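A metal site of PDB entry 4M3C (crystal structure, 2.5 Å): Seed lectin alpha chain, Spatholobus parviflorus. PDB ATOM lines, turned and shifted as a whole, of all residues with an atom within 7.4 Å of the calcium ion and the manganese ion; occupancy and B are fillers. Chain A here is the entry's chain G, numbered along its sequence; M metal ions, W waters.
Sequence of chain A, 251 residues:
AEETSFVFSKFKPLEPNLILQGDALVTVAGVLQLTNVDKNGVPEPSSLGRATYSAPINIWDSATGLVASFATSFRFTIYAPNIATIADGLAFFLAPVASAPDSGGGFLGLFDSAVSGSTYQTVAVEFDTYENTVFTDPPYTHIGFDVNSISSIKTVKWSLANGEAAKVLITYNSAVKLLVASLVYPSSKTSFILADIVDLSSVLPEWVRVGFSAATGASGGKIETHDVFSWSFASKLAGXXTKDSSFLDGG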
ATOM      1  N   ASP A  88      13.228  16.072 -25.224  1.00  0.00           N
ATOM      2  CA  ASP A  88      11.839  16.568 -25.128  1.00  0.00           C
ATOM      3  C   ASP A  88      11.185  16.535 -26.524  1.00  0.00           C
ATOM      4  O   ASP A  88       9.954  16.634 -26.625  1.00  0.00           O
ATOM      5  CB  ASP A  88      11.789  18.013 -24.609  1.00  0.00           C
ATOM      6  CG  ASP A  88      11.624  18.103 -23.088  1.00  0.00           C
ATOM      7  OD1 ASP A  88      12.606  17.825 -22.388  1.00  0.00           O
ATOM      8  OD2 ASP A  88      10.559  18.529 -22.582  1.00  0.00           O
ATOM      9  N   GLY A  89      11.995  16.438 -27.600  1.00  0.00           N
ATOM     10  CA  GLY A  89      11.482  16.210 -28.951  1.00  0.00           C
ATOM     11  C   GLY A  89      12.054  17.090 -30.038  1.00  0.00           C
ATOM     12  O   GLY A  89      12.942  17.900 -29.792  1.00  0.00           O
ATOM     13  N   GLY A 105      13.874  22.554 -23.381  1.00  0.00           N
ATOM     14  CA  GLY A 105      12.998  21.565 -22.718  1.00  0.00           C
ATOM     15  C   GLY A 105      11.714  21.456 -23.543  1.00  0.00           C
ATOM     16  O   GLY A 105      11.739  21.417 -24.777  1.00  0.00           O
ATOM     17  N   GLY A 106      10.564  21.470 -22.877  1.00  0.00           N
ATOM     18  CA  GLY A 106       9.312  21.207 -23.569  1.00  0.00           C
ATOM     19  C   GLY A 106       8.767  22.330 -24.429  1.00  0.00           C
ATOM     20  O   GLY A 106       7.717  22.170 -25.071  1.00  0.00           O
ATOM     21  N   PHE A 107       9.456  23.462 -24.465  1.00  0.00           N
ATOM     22  CA  PHE A 107       9.010  24.566 -25.294  1.00  0.00           C
ATOM     23  C   PHE A 107       9.616  24.368 -26.675  1.00  0.00           C
ATOM     24  O   PHE A 107       9.250  25.057 -27.620  1.00  0.00           O
ATOM     25  CB  PHE A 107       9.471  25.903 -24.741  1.00  0.00           C
ATOM     26  CG  PHE A 107       9.129  26.138 -23.299  1.00  0.00           C
ATOM     27  CD1 PHE A 107       7.918  26.723 -22.947  1.00  0.00           C
ATOM     28  CD2 PHE A 107      10.023  25.805 -22.299  1.00  0.00           C
ATOM     29  CE1 PHE A 107       7.600  26.951 -21.619  1.00  0.00           C
ATOM     30  CE2 PHE A 107       9.715  26.044 -20.973  1.00  0.00           C
ATOM     31  CZ  PHE A 107       8.499  26.622 -20.627  1.00  0.00           C
ATOM     32  N   LEU A 108      10.572  23.429 -26.750  1.00  0.00           N
ATOM     33  CA  LEU A 108      11.177  22.930 -28.008  1.00  0.00           C
ATOM     34  C   LEU A 108      11.832  24.011 -28.878  1.00  0.00           C
ATOM     35  O   LEU A 108      11.960  23.847 -30.099  1.00  0.00           O
ATOM     36  CB  LEU A 108      10.187  22.088 -28.819  1.00  0.00           C
ATOM     37  CG  LEU A 108       9.555  20.862 -28.176  1.00  0.00           C
ATOM     38  CD1 LEU A 108       8.470  20.298 -29.080  1.00  0.00           C
ATOM     39  CD2 LEU A 108      10.552  19.762 -27.862  1.00  0.00           C
ATOM     40  N   GLU A 126       5.123  19.199 -34.228  1.00  0.00           N
ATOM     41  CA  GLU A 126       5.984  18.689 -33.187  1.00  0.00           C
ATOM     42  C   GLU A 126       5.869  17.174 -33.107  1.00  0.00           C
ATOM     43  O   GLU A 126       4.807  16.605 -33.375  1.00  0.00           O
ATOM     44  CB  GLU A 126       5.672  19.311 -31.836  1.00  0.00           C
ATOM     45  CG  GLU A 126       4.261  19.106 -31.348  1.00  0.00           C
ATOM     46  CD  GLU A 126       4.104  19.383 -29.842  1.00  0.00           C
ATOM     47  OE1 GLU A 126       4.264  20.553 -29.394  1.00  0.00           O
ATOM     48  OE2 GLU A 126       3.811  18.403 -29.112  1.00  0.00           O
ATOM     49  N   PHE A 127       6.996  16.559 -32.764  1.00  0.00           N
ATOM     50  CA  PHE A 127       7.148  15.154 -32.640  1.00  0.00           C
ATOM     51  C   PHE A 127       7.683  15.056 -31.239  1.00  0.00           C
ATOM     52  O   PHE A 127       8.841  15.362 -30.984  1.00  0.00           O
ATOM     53  CB  PHE A 127       8.153  14.662 -33.671  1.00  0.00           C
ATOM     54  CG  PHE A 127       7.672  14.785 -35.090  1.00  0.00           C
ATOM     55  CD1 PHE A 127       6.994  13.725 -35.690  1.00  0.00           C
ATOM     56  CD2 PHE A 127       7.834  15.972 -35.803  1.00  0.00           C
ATOM     57  CE1 PHE A 127       6.503  13.840 -36.991  1.00  0.00           C
ATOM     58  CE2 PHE A 127       7.345  16.107 -37.094  1.00  0.00           C
ATOM     59  CZ  PHE A 127       6.686  15.038 -37.698  1.00  0.00           C
ATOM     60  N   ASP A 128       6.828  14.653 -30.308  1.00  0.00           N
ATOM     61  CA  ASP A 128       7.003  15.037 -28.908  1.00  0.00           C
ATOM     62  C   ASP A 128       7.005  13.834 -27.929  1.00  0.00           C
ATOM     63  O   ASP A 128       6.037  13.075 -27.849  1.00  0.00           O
ATOM     64  CB  ASP A 128       5.956  16.107 -28.555  1.00  0.00           C
ATOM     65  CG  ASP A 128       5.968  16.509 -27.100  1.00  0.00           C
ATOM     66  OD1 ASP A 128       6.833  16.053 -26.313  1.00  0.00           O
ATOM     67  OD2 ASP A 128       5.066  17.277 -26.720  1.00  0.00           O
ATOM     68  N   THR A 129       8.084  13.711 -27.174  1.00  0.00           N
ATOM     69  CA  THR A 129       8.472  12.460 -26.524  1.00  0.00           C
ATOM     70  C   THR A 129       8.294  12.443 -25.007  1.00  0.00           C
ATOM     71  O   THR A 129       8.381  11.391 -24.352  1.00  0.00           O
ATOM     72  CB  THR A 129       9.927  12.178 -26.864  1.00  0.00           C
ATOM     73  OG1 THR A 129      10.651  13.403 -26.761  1.00  0.00           O
ATOM     74  CG2 THR A 129      10.036  11.647 -28.334  1.00  0.00           C
ATOM     75  N   TYR A 130       7.998  13.624 -24.458  1.00  0.00           N
ATOM     76  CA  TYR A 130       7.873  13.778 -23.023  1.00  0.00           C
ATOM     77  C   TYR A 130       6.593  14.549 -22.711  1.00  0.00           C
ATOM     78  O   TYR A 130       6.356  15.644 -23.267  1.00  0.00           O
ATOM     79  CB  TYR A 130       9.115  14.511 -22.502  1.00  0.00           C
ATOM     80  CG  TYR A 130       9.062  14.772 -21.024  1.00  0.00           C
ATOM     81  CD1 TYR A 130       9.375  13.746 -20.096  1.00  0.00           C
ATOM     82  CD2 TYR A 130       8.686  16.020 -20.524  1.00  0.00           C
ATOM     83  CE1 TYR A 130       9.305  13.971 -18.734  1.00  0.00           C
ATOM     84  CE2 TYR A 130       8.610  16.251 -19.164  1.00  0.00           C
ATOM     85  CZ  TYR A 130       8.926  15.235 -18.267  1.00  0.00           C
ATOM     86  OH  TYR A 130       8.847  15.450 -16.903  1.00  0.00           O
ATOM     87  N   GLU A 131       5.778  13.983 -21.812  1.00  0.00           N
ATOM     88  CA  GLU A 131       4.551  14.620 -21.321  1.00  0.00           C
ATOM     89  C   GLU A 131       4.773  15.786 -20.338  1.00  0.00           C
ATOM     90  O   GLU A 131       5.201  15.601 -19.197  1.00  0.00           O
ATOM     91  CB  GLU A 131       3.578  13.590 -20.689  1.00  0.00           C
ATOM     92  CG  GLU A 131       2.226  14.226 -20.355  1.00  0.00           C
ATOM     93  CD  GLU A 131       1.276  13.369 -19.531  1.00  0.00           C
ATOM     94  OE1 GLU A 131       1.712  12.485 -18.740  1.00  0.00           O
ATOM     95  OE2 GLU A 131       0.053  13.605 -19.656  1.00  0.00           O
ATOM     96  N   ASN A 132       4.421  16.983 -20.785  1.00  0.00           N
ATOM     97  CA  ASN A 132       4.213  18.142 -19.921  1.00  0.00           C
ATOM     98  C   ASN A 132       2.727  18.347 -19.672  1.00  0.00           C
ATOM     99  O   ASN A 132       2.030  18.838 -20.563  1.00  0.00           O
ATOM    100  CB  ASN A 132       4.735  19.383 -20.616  1.00  0.00           C
ATOM    101  CG  ASN A 132       6.173  19.238 -20.998  1.00  0.00           C
ATOM    102  OD1 ASN A 132       6.513  18.712 -22.072  1.00  0.00           O
ATOM    103  ND2 ASN A 132       7.038  19.692 -20.107  1.00  0.00           N
ATOM    104  N   THR A 133       2.254  17.984 -18.486  1.00  0.00           N
ATOM    105  CA  THR A 133       0.811  18.126 -18.199  1.00  0.00           C
ATOM    106  C   THR A 133       0.470  19.592 -18.179  1.00  0.00           C
ATOM    107  O   THR A 133      -0.636  19.997 -18.485  1.00  0.00           O
ATOM    108  CB  THR A 133       0.364  17.473 -16.855  1.00  0.00           C
ATOM    109  OG1 THR A 133       1.195  17.953 -15.797  1.00  0.00           O
ATOM    110  CG2 THR A 133       0.473  15.984 -16.909  1.00  0.00           C
ATOM    111  N   PHE A 135       1.440  21.561 -20.337  1.00  0.00           N
ATOM    112  CA  PHE A 135       1.102  21.904 -21.744  1.00  0.00           C
ATOM    113  C   PHE A 135      -0.137  21.238 -22.361  1.00  0.00           C
ATOM    114  O   PHE A 135      -0.457  21.502 -23.537  1.00  0.00           O
ATOM    115  CB  PHE A 135       2.318  21.705 -22.676  1.00  0.00           C
ATOM    116  CG  PHE A 135       3.539  22.478 -22.253  1.00  0.00           C
ATOM    117  CD1 PHE A 135       3.437  23.584 -21.394  1.00  0.00           C
ATOM    118  CD2 PHE A 135       4.804  22.115 -22.728  1.00  0.00           C
ATOM    119  CE1 PHE A 135       4.580  24.307 -21.006  1.00  0.00           C
ATOM    120  CE2 PHE A 135       5.954  22.830 -22.338  1.00  0.00           C
ATOM    121  CZ  PHE A 135       5.842  23.926 -21.477  1.00  0.00           C
ATOM    122  N   THR A 136      -0.850  20.437 -21.561  1.00  0.00           N
ATOM    123  CA  THR A 136      -1.938  19.533 -22.005  1.00  0.00           C
ATOM    124  C   THR A 136      -1.431  18.381 -22.886  1.00  0.00           C
ATOM    125  O   THR A 136      -2.198  17.828 -23.654  1.00  0.00           O
ATOM    126  CB  THR A 136      -3.124  20.254 -22.696  1.00  0.00           C
ATOM    127  OG1 THR A 136      -3.322  21.533 -22.079  1.00  0.00           O
ATOM    128  CG2 THR A 136      -4.498  19.437 -22.577  1.00  0.00           C
ATOM    129  N   ASP A 137      -0.157  18.016 -22.771  1.00  0.00           N
ATOM    130  CA  ASP A 137       0.316  16.830 -23.486  1.00  0.00           C
ATOM    131  C   ASP A 137      -0.527  15.596 -23.112  1.00  0.00           C
ATOM    132  O   ASP A 137      -0.997  15.470 -22.012  1.00  0.00           O
ATOM    133  CB  ASP A 137       1.786  16.520 -23.193  1.00  0.00           C
ATOM    134  CG  ASP A 137       2.748  17.404 -23.922  1.00  0.00           C
ATOM    135  OD1 ASP A 137       2.371  18.172 -24.813  1.00  0.00           O
ATOM    136  OD2 ASP A 137       3.932  17.307 -23.583  1.00  0.00           O
ATOM    137  N   PRO A 138      -0.729  14.700 -24.079  1.00  0.00           N
ATOM    138  CA  PRO A 138      -1.293  13.396 -23.858  1.00  0.00           C
ATOM    139  C   PRO A 138      -0.298  12.545 -23.094  1.00  0.00           C
ATOM    140  O   PRO A 138       0.890  12.869 -23.103  1.00  0.00           O
ATOM    141  CB  PRO A 138      -1.407  12.829 -25.285  1.00  0.00           C
ATOM    142  CG  PRO A 138      -1.466  14.028 -26.163  1.00  0.00           C
ATOM    143  CD  PRO A 138      -0.509  14.970 -25.509  1.00  0.00           C
ATOM    144  N   TYR A 140       0.949   9.825 -23.829  1.00  0.00           N
ATOM    145  CA  TYR A 140       1.781   9.065 -24.760  1.00  0.00           C
ATOM    146  C   TYR A 140       2.623   9.984 -25.641  1.00  0.00           C
ATOM    147  O   TYR A 140       2.341  11.165 -25.782  1.00  0.00           O
ATOM    148  CB  TYR A 140       0.891   8.110 -25.605  1.00  0.00           C
ATOM    149  CG  TYR A 140      -0.410   8.736 -26.082  1.00  0.00           C
ATOM    150  CD1 TYR A 140      -0.413   9.600 -27.184  1.00  0.00           C
ATOM    151  CD2 TYR A 140      -1.634   8.486 -25.415  1.00  0.00           C
ATOM    152  CE1 TYR A 140      -1.593  10.187 -27.624  1.00  0.00           C
ATOM    153  CE2 TYR A 140      -2.820   9.070 -25.848  1.00  0.00           C
ATOM    154  CZ  TYR A 140      -2.803   9.924 -26.953  1.00  0.00           C
ATOM    155  OH  TYR A 140      -3.951  10.552 -27.431  1.00  0.00           O
ATOM    156  N   HIS A 142       3.508  11.739 -28.953  1.00  0.00           N
ATOM    157  CA  HIS A 142       2.509  12.210 -29.910  1.00  0.00           C
ATOM    158  C   HIS A 142       3.058  13.143 -30.938  1.00  0.00           C
ATOM    159  O   HIS A 142       4.057  13.814 -30.705  1.00  0.00           O
ATOM    160  CB  HIS A 142       1.415  12.891 -29.147  1.00  0.00           C
ATOM    161  CG  HIS A 142       1.921  13.995 -28.260  1.00  0.00           C
ATOM    162  ND1 HIS A 142       2.225  13.784 -26.995  1.00  0.00           N
ATOM    163  CD2 HIS A 142       2.216  15.319 -28.534  1.00  0.00           C
ATOM    164  CE1 HIS A 142       2.712  14.915 -26.465  1.00  0.00           C
ATOM    165  NE2 HIS A 142       2.687  15.858 -27.419  1.00  0.00           N
ATOM    166  N   ILE A 143       2.410  13.169 -32.101  1.00  0.00           N
ATOM    167  CA  ILE A 143       2.654  14.179 -33.168  1.00  0.00           C
ATOM    168  C   ILE A 143       1.597  15.263 -32.994  1.00  0.00           C
ATOM    169  O   ILE A 143       0.429  14.958 -32.784  1.00  0.00           O
ATOM    170  CB  ILE A 143       2.486  13.562 -34.564  1.00  0.00           C
ATOM    171  CG1 ILE A 143       3.593  12.519 -34.789  1.00  0.00           C
ATOM    172  CG2 ILE A 143       2.548  14.626 -35.638  1.00  0.00           C
ATOM    173  CD1 ILE A 143       3.229  11.411 -35.763  1.00  0.00           C
ATOM    174  N   GLY A 144       2.013  16.521 -33.065  1.00  0.00           N
ATOM    175  CA  GLY A 144       1.068  17.609 -32.727  1.00  0.00           C
ATOM    176  C   GLY A 144       1.189  18.820 -33.622  1.00  0.00           C
ATOM    177  O   GLY A 144       2.311  19.112 -34.122  1.00  0.00           O
ATOM    178  N   ASP A 146       1.249  22.748 -33.553  1.00  0.00           N
ATOM    179  CA  ASP A 146       1.489  23.911 -32.699  1.00  0.00           C
ATOM    180  C   ASP A 146       1.214  25.211 -33.510  1.00  0.00           C
ATOM    181  O   ASP A 146       1.901  25.512 -34.519  1.00  0.00           O
ATOM    182  CB  ASP A 146       2.934  23.867 -32.180  1.00  0.00           C
ATOM    183  CG  ASP A 146       3.209  22.680 -31.244  1.00  0.00           C
ATOM    184  OD1 ASP A 146       2.263  22.027 -30.774  1.00  0.00           O
ATOM    185  OD2 ASP A 146       4.394  22.406 -30.944  1.00  0.00           O
ATOM    186  N   ILE A 150       2.508  26.050 -27.554  1.00  0.00           N
ATOM    187  CA  ILE A 150       3.170  24.774 -27.409  1.00  0.00           C
ATOM    188  C   ILE A 150       2.082  23.810 -27.002  1.00  0.00           C
ATOM    189  O   ILE A 150       2.305  22.599 -26.848  1.00  0.00           O
ATOM    190  CB  ILE A 150       4.314  24.827 -26.345  1.00  0.00           C
ATOM    191  CG1 ILE A 150       5.095  23.513 -26.367  1.00  0.00           C
ATOM    192  CG2 ILE A 150       3.751  25.076 -24.952  1.00  0.00           C
ATOM    193  CD1 ILE A 150       5.861  23.260 -27.655  1.00  0.00           C
ATOM    194  N   SER A 151       0.898  24.399 -26.846  1.00  0.00           N
ATOM    195  CA  SER A 151      -0.312  23.677 -26.502  1.00  0.00           C
ATOM    196  C   SER A 151      -1.063  23.285 -27.774  1.00  0.00           C
ATOM    197  O   SER A 151      -1.965  23.979 -28.227  1.00  0.00           O
ATOM    198  CB  SER A 151      -1.171  24.564 -25.610  1.00  0.00           C
ATOM    199  OG  SER A 151      -2.348  23.882 -25.252  1.00  0.00           O
ATOM    200  N   SER A 152      -0.674  22.141 -28.335  1.00  0.00           N
ATOM    201  CA  SER A 152      -1.116  21.710 -29.663  1.00  0.00           C
ATOM    202  C   SER A 152      -2.583  21.897 -29.919  1.00  0.00           C
ATOM    203  O   SER A 152      -3.378  21.485 -29.092  1.00  0.00           O
ATOM    204  CB  SER A 152      -0.786  20.238 -29.821  1.00  0.00           C
ATOM    205  OG  SER A 152       0.603  20.054 -29.729  1.00  0.00           O
ATOM    206  N   THR A 155      -3.580  16.594 -31.644  1.00  0.00           N
ATOM    207  CA  THR A 155      -2.540  15.539 -31.550  1.00  0.00           C
ATOM    208  C   THR A 155      -3.005  14.135 -32.006  1.00  0.00           C
ATOM    209  O   THR A 155      -4.197  13.885 -32.094  1.00  0.00           O
ATOM    210  CB  THR A 155      -2.089  15.363 -30.097  1.00  0.00           C
ATOM    211  OG1 THR A 155      -3.191  14.838 -29.330  1.00  0.00           O
ATOM    212  CG2 THR A 155      -1.574  16.697 -29.498  1.00  0.00           C
HETATM  213 CA    CA M   1       6.122  17.818 -24.306  1.00  0.00          CA
HETATM  214 MN    MN M   2       3.179  17.919 -27.052  1.00  0.00          MN
HETATM  215  O   HOH W   1       6.098  19.921 -25.137  1.00  0.00           O
HETATM  216  O   HOH W   2       3.739  20.129 -26.958  1.00  0.00           O
HETATM  217  O   HOH W   3       0.701  18.681 -27.389  1.00  0.00           O
HETATM  218  O   HOH W   4       8.508  17.591 -24.764  1.00  0.00           O
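Water W2 lies within hydrogen-bond range of the side-chain carboxylate (OE1) of Glu 126 (2.5 Å) and the backbone carbonyl oxygen (O) of Ile 150 (2.9 Å).
The nearest printed residue that does not touch the manganese ion is Ser 152 (4.3 Å).
The manganese ion is bound by OD2 of Asp 128 (2.0 Å), NE2 of His 142 (2.2 Å), OE2 of Glu 126 (2.2 Å), water W2 (2.3 Å), OD1 of Asp 137 (2.4 Å) and water W3 (2.6 Å).
The manganese ion has six donor atoms within binding distance.
The side-chain carboxylate (OE1) of Glu 126 sits close to the side-chain carboxylate (OD2) of Asp 146, at 2.4 Å.
O of Glu 126 is in hydrogen-bond range of N of Gly 144 (2.8 Å).
A ring nitrogen (ND1) of His 142 lies within hydrogen-bond range of the backbone carbonyl oxygen of Tyr 140, 2.9 Å away.
The calcium ion is bound by water W1, the side-chain carboxylate (OD2) of Asp 137, the backbone carbonyl oxygen (O) of Tyr 130, the side-chain amide oxygen (OD1) of Asn 132, water W4, the side-chain carboxylate (OD2) of Asp 128 and the side-chain carboxylate (OD1) of Asp 128.
Of the 27 residues printed, 4 come within 4 Å of the calcium ion.
The nearest printed residue that does not touch the calcium ion is Glu 131 (4.6 Å).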
